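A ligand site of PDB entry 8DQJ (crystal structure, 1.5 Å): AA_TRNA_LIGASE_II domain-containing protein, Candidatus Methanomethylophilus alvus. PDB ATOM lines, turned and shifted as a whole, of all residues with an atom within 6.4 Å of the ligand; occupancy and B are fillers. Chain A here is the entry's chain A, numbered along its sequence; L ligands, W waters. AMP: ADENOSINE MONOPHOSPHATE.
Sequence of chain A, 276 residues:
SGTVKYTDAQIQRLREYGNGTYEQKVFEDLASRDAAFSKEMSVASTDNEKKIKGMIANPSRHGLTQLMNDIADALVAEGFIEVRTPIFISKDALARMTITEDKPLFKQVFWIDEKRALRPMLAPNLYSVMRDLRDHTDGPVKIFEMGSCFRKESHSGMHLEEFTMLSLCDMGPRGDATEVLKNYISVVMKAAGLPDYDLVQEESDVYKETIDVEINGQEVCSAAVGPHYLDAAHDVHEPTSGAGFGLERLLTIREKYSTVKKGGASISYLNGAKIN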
ATOM      1  N   GLN A 108     -24.861  -8.805   6.031  1.00  0.00           N
ATOM      2  CA  GLN A 108     -23.749  -9.654   5.627  1.00  0.00           C
ATOM      3  C   GLN A 108     -23.729  -9.949   4.138  1.00  0.00           C
ATOM      4  O   GLN A 108     -22.843 -10.679   3.685  1.00  0.00           O
ATOM      5  CB  GLN A 108     -23.799 -10.987   6.382  1.00  0.00           C
ATOM      6  CG  GLN A 108     -23.738 -10.918   7.897  1.00  0.00           C
ATOM      7  CD  GLN A 108     -23.665 -12.300   8.510  1.00  0.00           C
ATOM      8  OE1 GLN A 108     -24.666 -12.876   8.907  1.00  0.00           O
ATOM      9  NE2 GLN A 108     -22.452 -12.852   8.554  1.00  0.00           N
ATOM     10  N   PRO A 120     -26.154 -15.889  -0.033  1.00  0.00           N
ATOM     11  CA  PRO A 120     -25.602 -16.246   1.283  1.00  0.00           C
ATOM     12  C   PRO A 120     -26.020 -17.630   1.767  1.00  0.00           C
ATOM     13  O   PRO A 120     -25.516 -18.090   2.804  1.00  0.00           O
ATOM     14  CB  PRO A 120     -26.174 -15.147   2.203  1.00  0.00           C
ATOM     15  CG  PRO A 120     -27.477 -14.797   1.609  1.00  0.00           C
ATOM     16  CD  PRO A 120     -27.338 -15.019   0.094  1.00  0.00           C
ATOM     17  N   MET A 121     -26.885 -18.299   1.006  1.00  0.00           N
ATOM     18  CA  MET A 121     -27.391 -19.634   1.332  1.00  0.00           C
ATOM     19  C   MET A 121     -27.961 -20.203   0.040  1.00  0.00           C
ATOM     20  O   MET A 121     -28.247 -19.475  -0.907  1.00  0.00           O
ATOM     21  CB  MET A 121     -28.447 -19.583   2.436  1.00  0.00           C
ATOM     22  CG  MET A 121     -29.511 -18.538   2.201  1.00  0.00           C
ATOM     23  SD  MET A 121     -30.900 -18.731   3.334  1.00  0.00           S
ATOM     24  CE  MET A 121     -30.128 -18.455   4.922  1.00  0.00           C
ATOM     25  N   ARG A 151     -20.735 -14.575   2.698  1.00  0.00           N
ATOM     26  CA  ARG A 151     -21.234 -13.695   3.753  1.00  0.00           C
ATOM     27  C   ARG A 151     -20.097 -12.840   4.292  1.00  0.00           C
ATOM     28  O   ARG A 151     -18.989 -13.346   4.529  1.00  0.00           O
ATOM     29  CB  ARG A 151     -21.855 -14.458   4.934  1.00  0.00           C
ATOM     30  CG  ARG A 151     -23.022 -15.362   4.553  1.00  0.00           C
ATOM     31  CD  ARG A 151     -23.645 -16.017   5.775  1.00  0.00           C
ATOM     32  NE  ARG A 151     -24.548 -17.102   5.376  1.00  0.00           N
ATOM     33  CZ  ARG A 151     -25.224 -17.872   6.213  1.00  0.00           C
ATOM     34  NH1 ARG A 151     -25.207 -17.673   7.526  1.00  0.00           N
ATOM     35  NH2 ARG A 151     -25.959 -18.874   5.725  1.00  0.00           N
ATOM     36  N   GLU A 153     -17.873 -11.286   6.933  1.00  0.00           N
ATOM     37  CA  GLU A 153     -17.553 -11.758   8.283  1.00  0.00           C
ATOM     38  C   GLU A 153     -16.538 -10.851   8.979  1.00  0.00           C
ATOM     39  O   GLU A 153     -15.733 -10.197   8.321  1.00  0.00           O
ATOM     40  CB  GLU A 153     -17.012 -13.203   8.218  1.00  0.00           C
ATOM     41  CG  GLU A 153     -18.014 -14.242   7.676  1.00  0.00           C
ATOM     42  CD  GLU A 153     -19.219 -14.433   8.608  1.00  0.00           C
ATOM     43  OE1 GLU A 153     -19.065 -14.243   9.834  1.00  0.00           O
ATOM     44  OE2 GLU A 153     -20.300 -14.779   8.112  1.00  0.00           O
ATOM     45  N   LEU A 160     -15.445 -18.057   7.550  1.00  0.00           N
ATOM     46  CA  LEU A 160     -15.054 -17.923   6.139  1.00  0.00           C
ATOM     47  C   LEU A 160     -16.020 -17.019   5.377  1.00  0.00           C
ATOM     48  O   LEU A 160     -17.231 -17.186   5.503  1.00  0.00           O
ATOM     49  CB  LEU A 160     -15.043 -19.307   5.460  1.00  0.00           C
ATOM     50  CG  LEU A 160     -14.140 -20.427   5.979  1.00  0.00           C
ATOM     51  CD1 LEU A 160     -14.493 -21.737   5.240  1.00  0.00           C
ATOM     52  CD2 LEU A 160     -12.695 -20.066   5.756  1.00  0.00           C
ATOM     53  N   GLU A 161     -15.516 -16.104   4.546  1.00  0.00           N
ATOM     54  CA  GLU A 161     -16.414 -15.274   3.761  1.00  0.00           C
ATOM     55  C   GLU A 161     -16.983 -16.037   2.566  1.00  0.00           C
ATOM     56  O   GLU A 161     -18.104 -15.767   2.145  1.00  0.00           O
ATOM     57  CB  GLU A 161     -15.699 -13.995   3.282  1.00  0.00           C
ATOM     58  CG  GLU A 161     -15.348 -13.044   4.418  1.00  0.00           C
ATOM     59  CD  GLU A 161     -15.224 -11.574   3.990  1.00  0.00           C
ATOM     60  OE1 GLU A 161     -14.669 -11.294   2.913  1.00  0.00           O
ATOM     61  OE2 GLU A 161     -15.683 -10.700   4.760  1.00  0.00           O
ATOM     62  N   GLU A 162     -16.221 -16.979   2.025  1.00  0.00           N
ATOM     63  CA  GLU A 162     -16.704 -17.925   1.005  1.00  0.00           C
ATOM     64  C   GLU A 162     -16.662 -19.317   1.644  1.00  0.00           C
ATOM     65  O   GLU A 162     -15.613 -19.727   2.153  1.00  0.00           O
ATOM     66  CB  GLU A 162     -15.850 -17.905  -0.278  1.00  0.00           C
ATOM     67  CG  GLU A 162     -16.279 -19.008  -1.256  1.00  0.00           C
ATOM     68  CD  GLU A 162     -15.418 -19.107  -2.476  1.00  0.00           C
ATOM     69  OE1 GLU A 162     -14.399 -18.374  -2.584  1.00  0.00           O
ATOM     70  OE2 GLU A 162     -15.761 -19.954  -3.338  1.00  0.00           O
ATOM     71  N   PHE A 163     -17.790 -20.024   1.637  1.00  0.00           N
ATOM     72  CA  PHE A 163     -17.864 -21.345   2.237  1.00  0.00           C
ATOM     73  C   PHE A 163     -18.719 -22.220   1.327  1.00  0.00           C
ATOM     74  O   PHE A 163     -19.469 -21.714   0.477  1.00  0.00           O
ATOM     75  CB  PHE A 163     -18.416 -21.309   3.691  1.00  0.00           C
ATOM     76  CG  PHE A 163     -19.776 -20.713   3.821  1.00  0.00           C
ATOM     77  CD1 PHE A 163     -19.940 -19.329   3.869  1.00  0.00           C
ATOM     78  CD2 PHE A 163     -20.900 -21.530   3.876  1.00  0.00           C
ATOM     79  CE1 PHE A 163     -21.196 -18.771   3.957  1.00  0.00           C
ATOM     80  CE2 PHE A 163     -22.144 -20.973   3.985  1.00  0.00           C
ATOM     81  CZ  PHE A 163     -22.285 -19.584   4.002  1.00  0.00           C
ATOM     82  N   THR A 164     -18.623 -23.526   1.490  1.00  0.00           N
ATOM     83  CA  THR A 164     -19.318 -24.458   0.591  1.00  0.00           C
ATOM     84  C   THR A 164     -20.453 -25.069   1.398  1.00  0.00           C
ATOM     85  O   THR A 164     -20.225 -25.796   2.377  1.00  0.00           O
ATOM     86  CB  THR A 164     -18.392 -25.526   0.040  1.00  0.00           C
ATOM     87  OG1 THR A 164     -17.205 -24.912  -0.488  1.00  0.00           O
ATOM     88  CG2 THR A 164     -19.082 -26.281  -1.106  1.00  0.00           C
ATOM     89  N   MET A 165     -21.682 -24.781   0.988  1.00  0.00           N
ATOM     90  CA  MET A 165     -22.851 -25.367   1.610  1.00  0.00           C
ATOM     91  C   MET A 165     -23.288 -26.593   0.821  1.00  0.00           C
ATOM     92  O   MET A 165     -23.150 -26.634  -0.416  1.00  0.00           O
ATOM     93  CB  MET A 165     -23.981 -24.332   1.701  1.00  0.00           C
ATOM     94  CG  MET A 165     -25.066 -24.589   2.750  1.00  0.00           C
ATOM     95  SD  MET A 165     -26.384 -23.334   2.809  1.00  0.00           S
ATOM     96  CE  MET A 165     -25.504 -21.931   3.491  1.00  0.00           C
ATOM     97  N   ASP A 212     -30.451 -28.758  14.973  1.00  0.00           N
ATOM     98  CA  ASP A 212     -29.048 -28.462  14.696  1.00  0.00           C
ATOM     99  C   ASP A 212     -28.212 -29.717  14.930  1.00  0.00           C
ATOM    100  O   ASP A 212     -28.462 -30.478  15.861  1.00  0.00           O
ATOM    101  CB  ASP A 212     -28.542 -27.314  15.550  1.00  0.00           C
ATOM    102  CG  ASP A 212     -29.035 -25.960  15.059  1.00  0.00           C
ATOM    103  OD1 ASP A 212     -29.545 -25.861  13.925  1.00  0.00           O
ATOM    104  OD2 ASP A 212     -28.909 -24.976  15.830  1.00  0.00           O
ATOM    105  N   VAL A 213     -27.196 -29.878  14.094  1.00  0.00           N
ATOM    106  CA  VAL A 213     -26.222 -30.954  14.219  1.00  0.00           C
ATOM    107  C   VAL A 213     -24.957 -30.359  14.790  1.00  0.00           C
ATOM    108  O   VAL A 213     -24.411 -29.404  14.223  1.00  0.00           O
ATOM    109  CB  VAL A 213     -25.944 -31.638  12.877  1.00  0.00           C
ATOM    110  CG1 VAL A 213     -25.109 -32.889  13.074  1.00  0.00           C
ATOM    111  CG2 VAL A 213     -27.262 -31.939  12.160  1.00  0.00           C
ATOM    112  N   GLU A 219     -21.538 -26.325  15.705  1.00  0.00           N
ATOM    113  CA  GLU A 219     -22.629 -26.552  14.767  1.00  0.00           C
ATOM    114  C   GLU A 219     -22.071 -26.777  13.364  1.00  0.00           C
ATOM    115  O   GLU A 219     -21.253 -25.981  12.876  1.00  0.00           O
ATOM    116  CB  GLU A 219     -23.597 -25.367  14.776  1.00  0.00           C
ATOM    117  CG  GLU A 219     -24.841 -25.575  13.902  1.00  0.00           C
ATOM    118  CD  GLU A 219     -25.417 -24.281  13.364  1.00  0.00           C
ATOM    119  OE1 GLU A 219     -25.786 -23.400  14.178  1.00  0.00           O
ATOM    120  OE2 GLU A 219     -25.487 -24.117  12.129  1.00  0.00           O
ATOM    121  N   VAL A 220     -22.517 -27.852  12.730  1.00  0.00           N
ATOM    122  CA  VAL A 220     -22.115 -28.186  11.370  1.00  0.00           C
ATOM    123  C   VAL A 220     -23.299 -28.257  10.423  1.00  0.00           C
ATOM    124  O   VAL A 220     -23.098 -28.335   9.191  1.00  0.00           O
ATOM    125  CB  VAL A 220     -21.346 -29.518  11.329  1.00  0.00           C
ATOM    126  CG1 VAL A 220     -20.051 -29.406  12.113  1.00  0.00           C
ATOM    127  CG2 VAL A 220     -22.218 -30.641  11.890  1.00  0.00           C
ATOM    128  N   CYS A 221     -24.524 -28.261  10.940  1.00  0.00           N
ATOM    129  CA  CYS A 221     -25.720 -28.338  10.097  1.00  0.00           C
ATOM    130  C   CYS A 221     -26.896 -27.711  10.834  1.00  0.00           C
ATOM    131  O   CYS A 221     -27.021 -27.880  12.061  1.00  0.00           O
ATOM    132  CB  CYS A 221     -26.062 -29.792   9.734  1.00  0.00           C
ATOM    133  SG  CYS A 221     -27.758 -30.010   9.037  1.00  0.00           S
ATOM    134  N   SER A 222     -27.743 -27.016  10.091  1.00  0.00           N
ATOM    135  CA  SER A 222     -29.038 -26.550  10.590  1.00  0.00           C
ATOM    136  C   SER A 222     -30.110 -27.083   9.657  1.00  0.00           C
ATOM    137  O   SER A 222     -30.004 -26.922   8.440  1.00  0.00           O
ATOM    138  CB  SER A 222     -29.123 -25.029  10.681  1.00  0.00           C
ATOM    139  OG  SER A 222     -29.244 -24.450   9.394  1.00  0.00           O
ATOM    140  N   GLY A 244     -28.988 -27.916   5.842  1.00  0.00           N
ATOM    141  CA  GLY A 244     -27.839 -27.232   5.308  1.00  0.00           C
ATOM    142  C   GLY A 244     -26.591 -27.520   6.110  1.00  0.00           C
ATOM    143  O   GLY A 244     -26.567 -27.307   7.317  1.00  0.00           O
ATOM    144  N   PHE A 245     -25.535 -27.987   5.445  1.00  0.00           N
ATOM    145  CA  PHE A 245     -24.292 -28.382   6.076  1.00  0.00           C
ATOM    146  C   PHE A 245     -23.169 -27.461   5.597  1.00  0.00           C
ATOM    147  O   PHE A 245     -23.120 -27.082   4.420  1.00  0.00           O
ATOM    148  CB  PHE A 245     -23.894 -29.838   5.739  1.00  0.00           C
ATOM    149  CG  PHE A 245     -24.918 -30.871   6.100  1.00  0.00           C
ATOM    150  CD1 PHE A 245     -26.065 -31.011   5.334  1.00  0.00           C
ATOM    151  CD2 PHE A 245     -24.710 -31.744   7.180  1.00  0.00           C
ATOM    152  CE1 PHE A 245     -27.033 -31.959   5.649  1.00  0.00           C
ATOM    153  CE2 PHE A 245     -25.650 -32.703   7.489  1.00  0.00           C
ATOM    154  CZ  PHE A 245     -26.809 -32.813   6.732  1.00  0.00           C
ATOM    155  N   GLY A 246     -22.237 -27.138   6.494  1.00  0.00           N
ATOM    156  CA  GLY A 246     -21.036 -26.438   6.076  1.00  0.00           C
ATOM    157  C   GLY A 246     -19.927 -27.440   5.810  1.00  0.00           C
ATOM    158  O   GLY A 246     -19.422 -28.066   6.748  1.00  0.00           O
ATOM    159  N   LEU A 247     -19.535 -27.591   4.547  1.00  0.00           N
ATOM    160  CA  LEU A 247     -18.659 -28.697   4.205  1.00  0.00           C
ATOM    161  C   LEU A 247     -17.223 -28.461   4.660  1.00  0.00           C
ATOM    162  O   LEU A 247     -16.546 -29.422   5.046  1.00  0.00           O
ATOM    163  CB  LEU A 247     -18.673 -28.954   2.708  1.00  0.00           C
ATOM    164  CG  LEU A 247     -20.023 -29.547   2.288  1.00  0.00           C
ATOM    165  CD1 LEU A 247     -19.922 -29.783   0.794  1.00  0.00           C
ATOM    166  CD2 LEU A 247     -20.455 -30.814   3.045  1.00  0.00           C
ATOM    167  N   GLU A 248     -16.729 -27.219   4.626  1.00  0.00           N
ATOM    168  CA  GLU A 248     -15.397 -26.978   5.181  1.00  0.00           C
ATOM    169  C   GLU A 248     -15.379 -27.318   6.665  1.00  0.00           C
ATOM    170  O   GLU A 248     -14.386 -27.871   7.161  1.00  0.00           O
ATOM    171  CB  GLU A 248     -14.947 -25.520   4.983  1.00  0.00           C
ATOM    172  CG  GLU A 248     -14.618 -25.150   3.549  1.00  0.00           C
ATOM    173  CD  GLU A 248     -15.830 -24.678   2.789  1.00  0.00           C
ATOM    174  OE1 GLU A 248     -16.949 -24.628   3.381  1.00  0.00           O
ATOM    175  OE2 GLU A 248     -15.649 -24.368   1.576  1.00  0.00           O
ATOM    176  N   ARG A 249     -16.443 -26.998   7.402  1.00  0.00           N
ATOM    177  CA  ARG A 249     -16.491 -27.338   8.824  1.00  0.00           C
ATOM    178  C   ARG A 249     -16.426 -28.840   9.036  1.00  0.00           C
ATOM    179  O   ARG A 249     -15.705 -29.319   9.918  1.00  0.00           O
ATOM    180  CB  ARG A 249     -17.750 -26.764   9.491  1.00  0.00           C
ATOM    181  CG  ARG A 249     -17.749 -25.256   9.594  1.00  0.00           C
ATOM    182  CD  ARG A 249     -18.866 -24.735  10.498  1.00  0.00           C
ATOM    183  NE  ARG A 249     -18.847 -23.281  10.568  1.00  0.00           N
ATOM    184  CZ  ARG A 249     -19.769 -22.540  11.160  1.00  0.00           C
ATOM    185  NH1 ARG A 249     -20.824 -23.079  11.749  1.00  0.00           N
ATOM    186  NH2 ARG A 249     -19.634 -21.212  11.173  1.00  0.00           N
ATOM    187  N   VAL A 260     -10.246 -23.597  10.375  1.00  0.00           N
ATOM    188  CA  VAL A 260     -11.172 -23.901   9.284  1.00  0.00           C
ATOM    189  C   VAL A 260     -10.697 -23.389   7.931  1.00  0.00           C
ATOM    190  O   VAL A 260     -11.414 -23.561   6.941  1.00  0.00           O
ATOM    191  CB  VAL A 260     -12.571 -23.311   9.585  1.00  0.00           C
ATOM    192  CG1 VAL A 260     -12.516 -21.778   9.518  1.00  0.00           C
ATOM    193  CG2 VAL A 260     -13.629 -23.893   8.655  1.00  0.00           C
HETATM  194  P   AMP L   1     -27.137 -21.194   8.242  1.00  0.00           P
HETATM  195  O1P AMP L   1     -27.779 -21.967   9.369  1.00  0.00           O
HETATM  196  O2P AMP L   1     -26.542 -19.870   8.648  1.00  0.00           O
HETATM  197  O3P AMP L   1     -27.945 -21.133   6.955  1.00  0.00           O
HETATM  198  O5' AMP L   1     -25.857 -22.053   7.837  1.00  0.00           O
HETATM  199  C5' AMP L   1     -25.939 -23.453   7.627  1.00  0.00           C
HETATM  200  C4' AMP L   1     -24.580 -24.084   7.818  1.00  0.00           C
HETATM  201  O4' AMP L   1     -23.634 -23.405   6.956  1.00  0.00           O
HETATM  202  C3' AMP L   1     -24.006 -23.930   9.215  1.00  0.00           C
HETATM  203  O3' AMP L   1     -24.449 -24.937  10.115  1.00  0.00           O
HETATM  204  C2' AMP L   1     -22.494 -23.933   8.987  1.00  0.00           C
HETATM  205  O2' AMP L   1     -21.969 -25.250   8.979  1.00  0.00           O
HETATM  206  C1' AMP L   1     -22.369 -23.341   7.572  1.00  0.00           C
HETATM  207  N9  AMP L   1     -21.941 -21.929   7.590  1.00  0.00           N
HETATM  208  C8  AMP L   1     -22.740 -20.854   7.709  1.00  0.00           C
HETATM  209  N7  AMP L   1     -22.023 -19.709   7.676  1.00  0.00           N
HETATM  210  C5  AMP L   1     -20.730 -20.063   7.508  1.00  0.00           C
HETATM  211  C6  AMP L   1     -19.445 -19.354   7.381  1.00  0.00           C
HETATM  212  N6  AMP L   1     -19.403 -17.995   7.429  1.00  0.00           N
HETATM  213  N1  AMP L   1     -18.333 -20.105   7.231  1.00  0.00           N
HETATM  214  C2  AMP L   1     -18.356 -21.454   7.186  1.00  0.00           C
HETATM  215  N3  AMP L   1     -19.488 -22.163   7.289  1.00  0.00           N
HETATM  216  C4  AMP L   1     -20.680 -21.527   7.449  1.00  0.00           C
HETATM  217  O   HOH W   1     -18.286 -24.769   6.071  1.00  0.00           O
HETATM  218  O   HOH W   2     -24.947 -19.374  10.772  1.00  0.00           O
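N6 of the ligand is in hydrogen-bond range of OE2 of Glu 153 (3.4 Å).
The backbone NH (N) of Gly 246 sits at hydrogen-bond distance from an oxygen (O2') of the ligand (3.1 Å).
OE2 of Glu 219 sits at hydrogen-bond distance from O3' of the ligand, 2.4 Å away.
OG of Ser 222 lies within hydrogen-bond range of O1P of the ligand (2.9 Å).
An oxygen (O2P) of the ligand is in salt-bridge range of the guanidinium group (NH1) of Arg 151 (2.8 Å).
The backbone carbonyl oxygen of Val 220 is in hydrogen-bond range of an oxygen (O2') of the ligand (3.3 Å).
O of Leu 160 sits at hydrogen-bond distance from N6 of the ligand (3.0 Å).
N of Cys 221 lies within hydrogen-bond range of O3' of the ligand (3.4 Å).
The backbone NH of Val 213 is in hydrogen-bond range of the backbone carbonyl oxygen of Cys 221, at 2.9 Å.
The backbone NH of Val 220 sits at hydrogen-bond distance from the backbone carbonyl oxygen of Val 213 (2.9 Å).
The backbone carbonyl oxygen of Glu 219 lies within hydrogen-bond range of the guanidinium group of Arg 249 (3.1 Å).
O of Pro 120 sits at hydrogen-bond distance from NE of Arg 151, at 2.9 Å.
The backbone NH (N) of Glu 153 is in hydrogen-bond range of the side-chain carboxylate (OE2) of Glu 161 (3.1 Å).
N of Gly 246 lies within hydrogen-bond range of O of Val 220, at 3.1 Å.
The backbone carbonyl oxygen (O) of Glu 161 lies within hydrogen-bond range of the backbone NH (N) of Arg 151 (2.9 Å).
NE2 of Gln 108 is in hydrogen-bond range of OE2 of Glu 153.
Phe 163 touches the ligand (CB to C2, 3.5 Å).
Gly 244 touches the ligand.
Arg 249 touches the ligand (NH1 to C2', 3.3 Å).
Hydrophobic or aromatic side chains within 4 Å of the ligand: Leu 160 and Phe 163.
Within 4 Å of the ligand: Arg 151, Glu 153, Leu 160, Phe 163, Glu 219, Val 220, Cys 221, Ser 222, Gly 244, Gly 246 and Arg 249.
The nearest printed residue that does not touch the ligand is Met 121 (4.01 Å).
Water W1 lies within hydrogen-bond range of the side-chain carboxylate of Glu 248 (3.0 Å), a nitrogen (N3) of the ligand (3.1 Å), the backbone NH of Arg 249 (3.2 Å) and the backbone NH of Leu 247 (3.4 Å).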
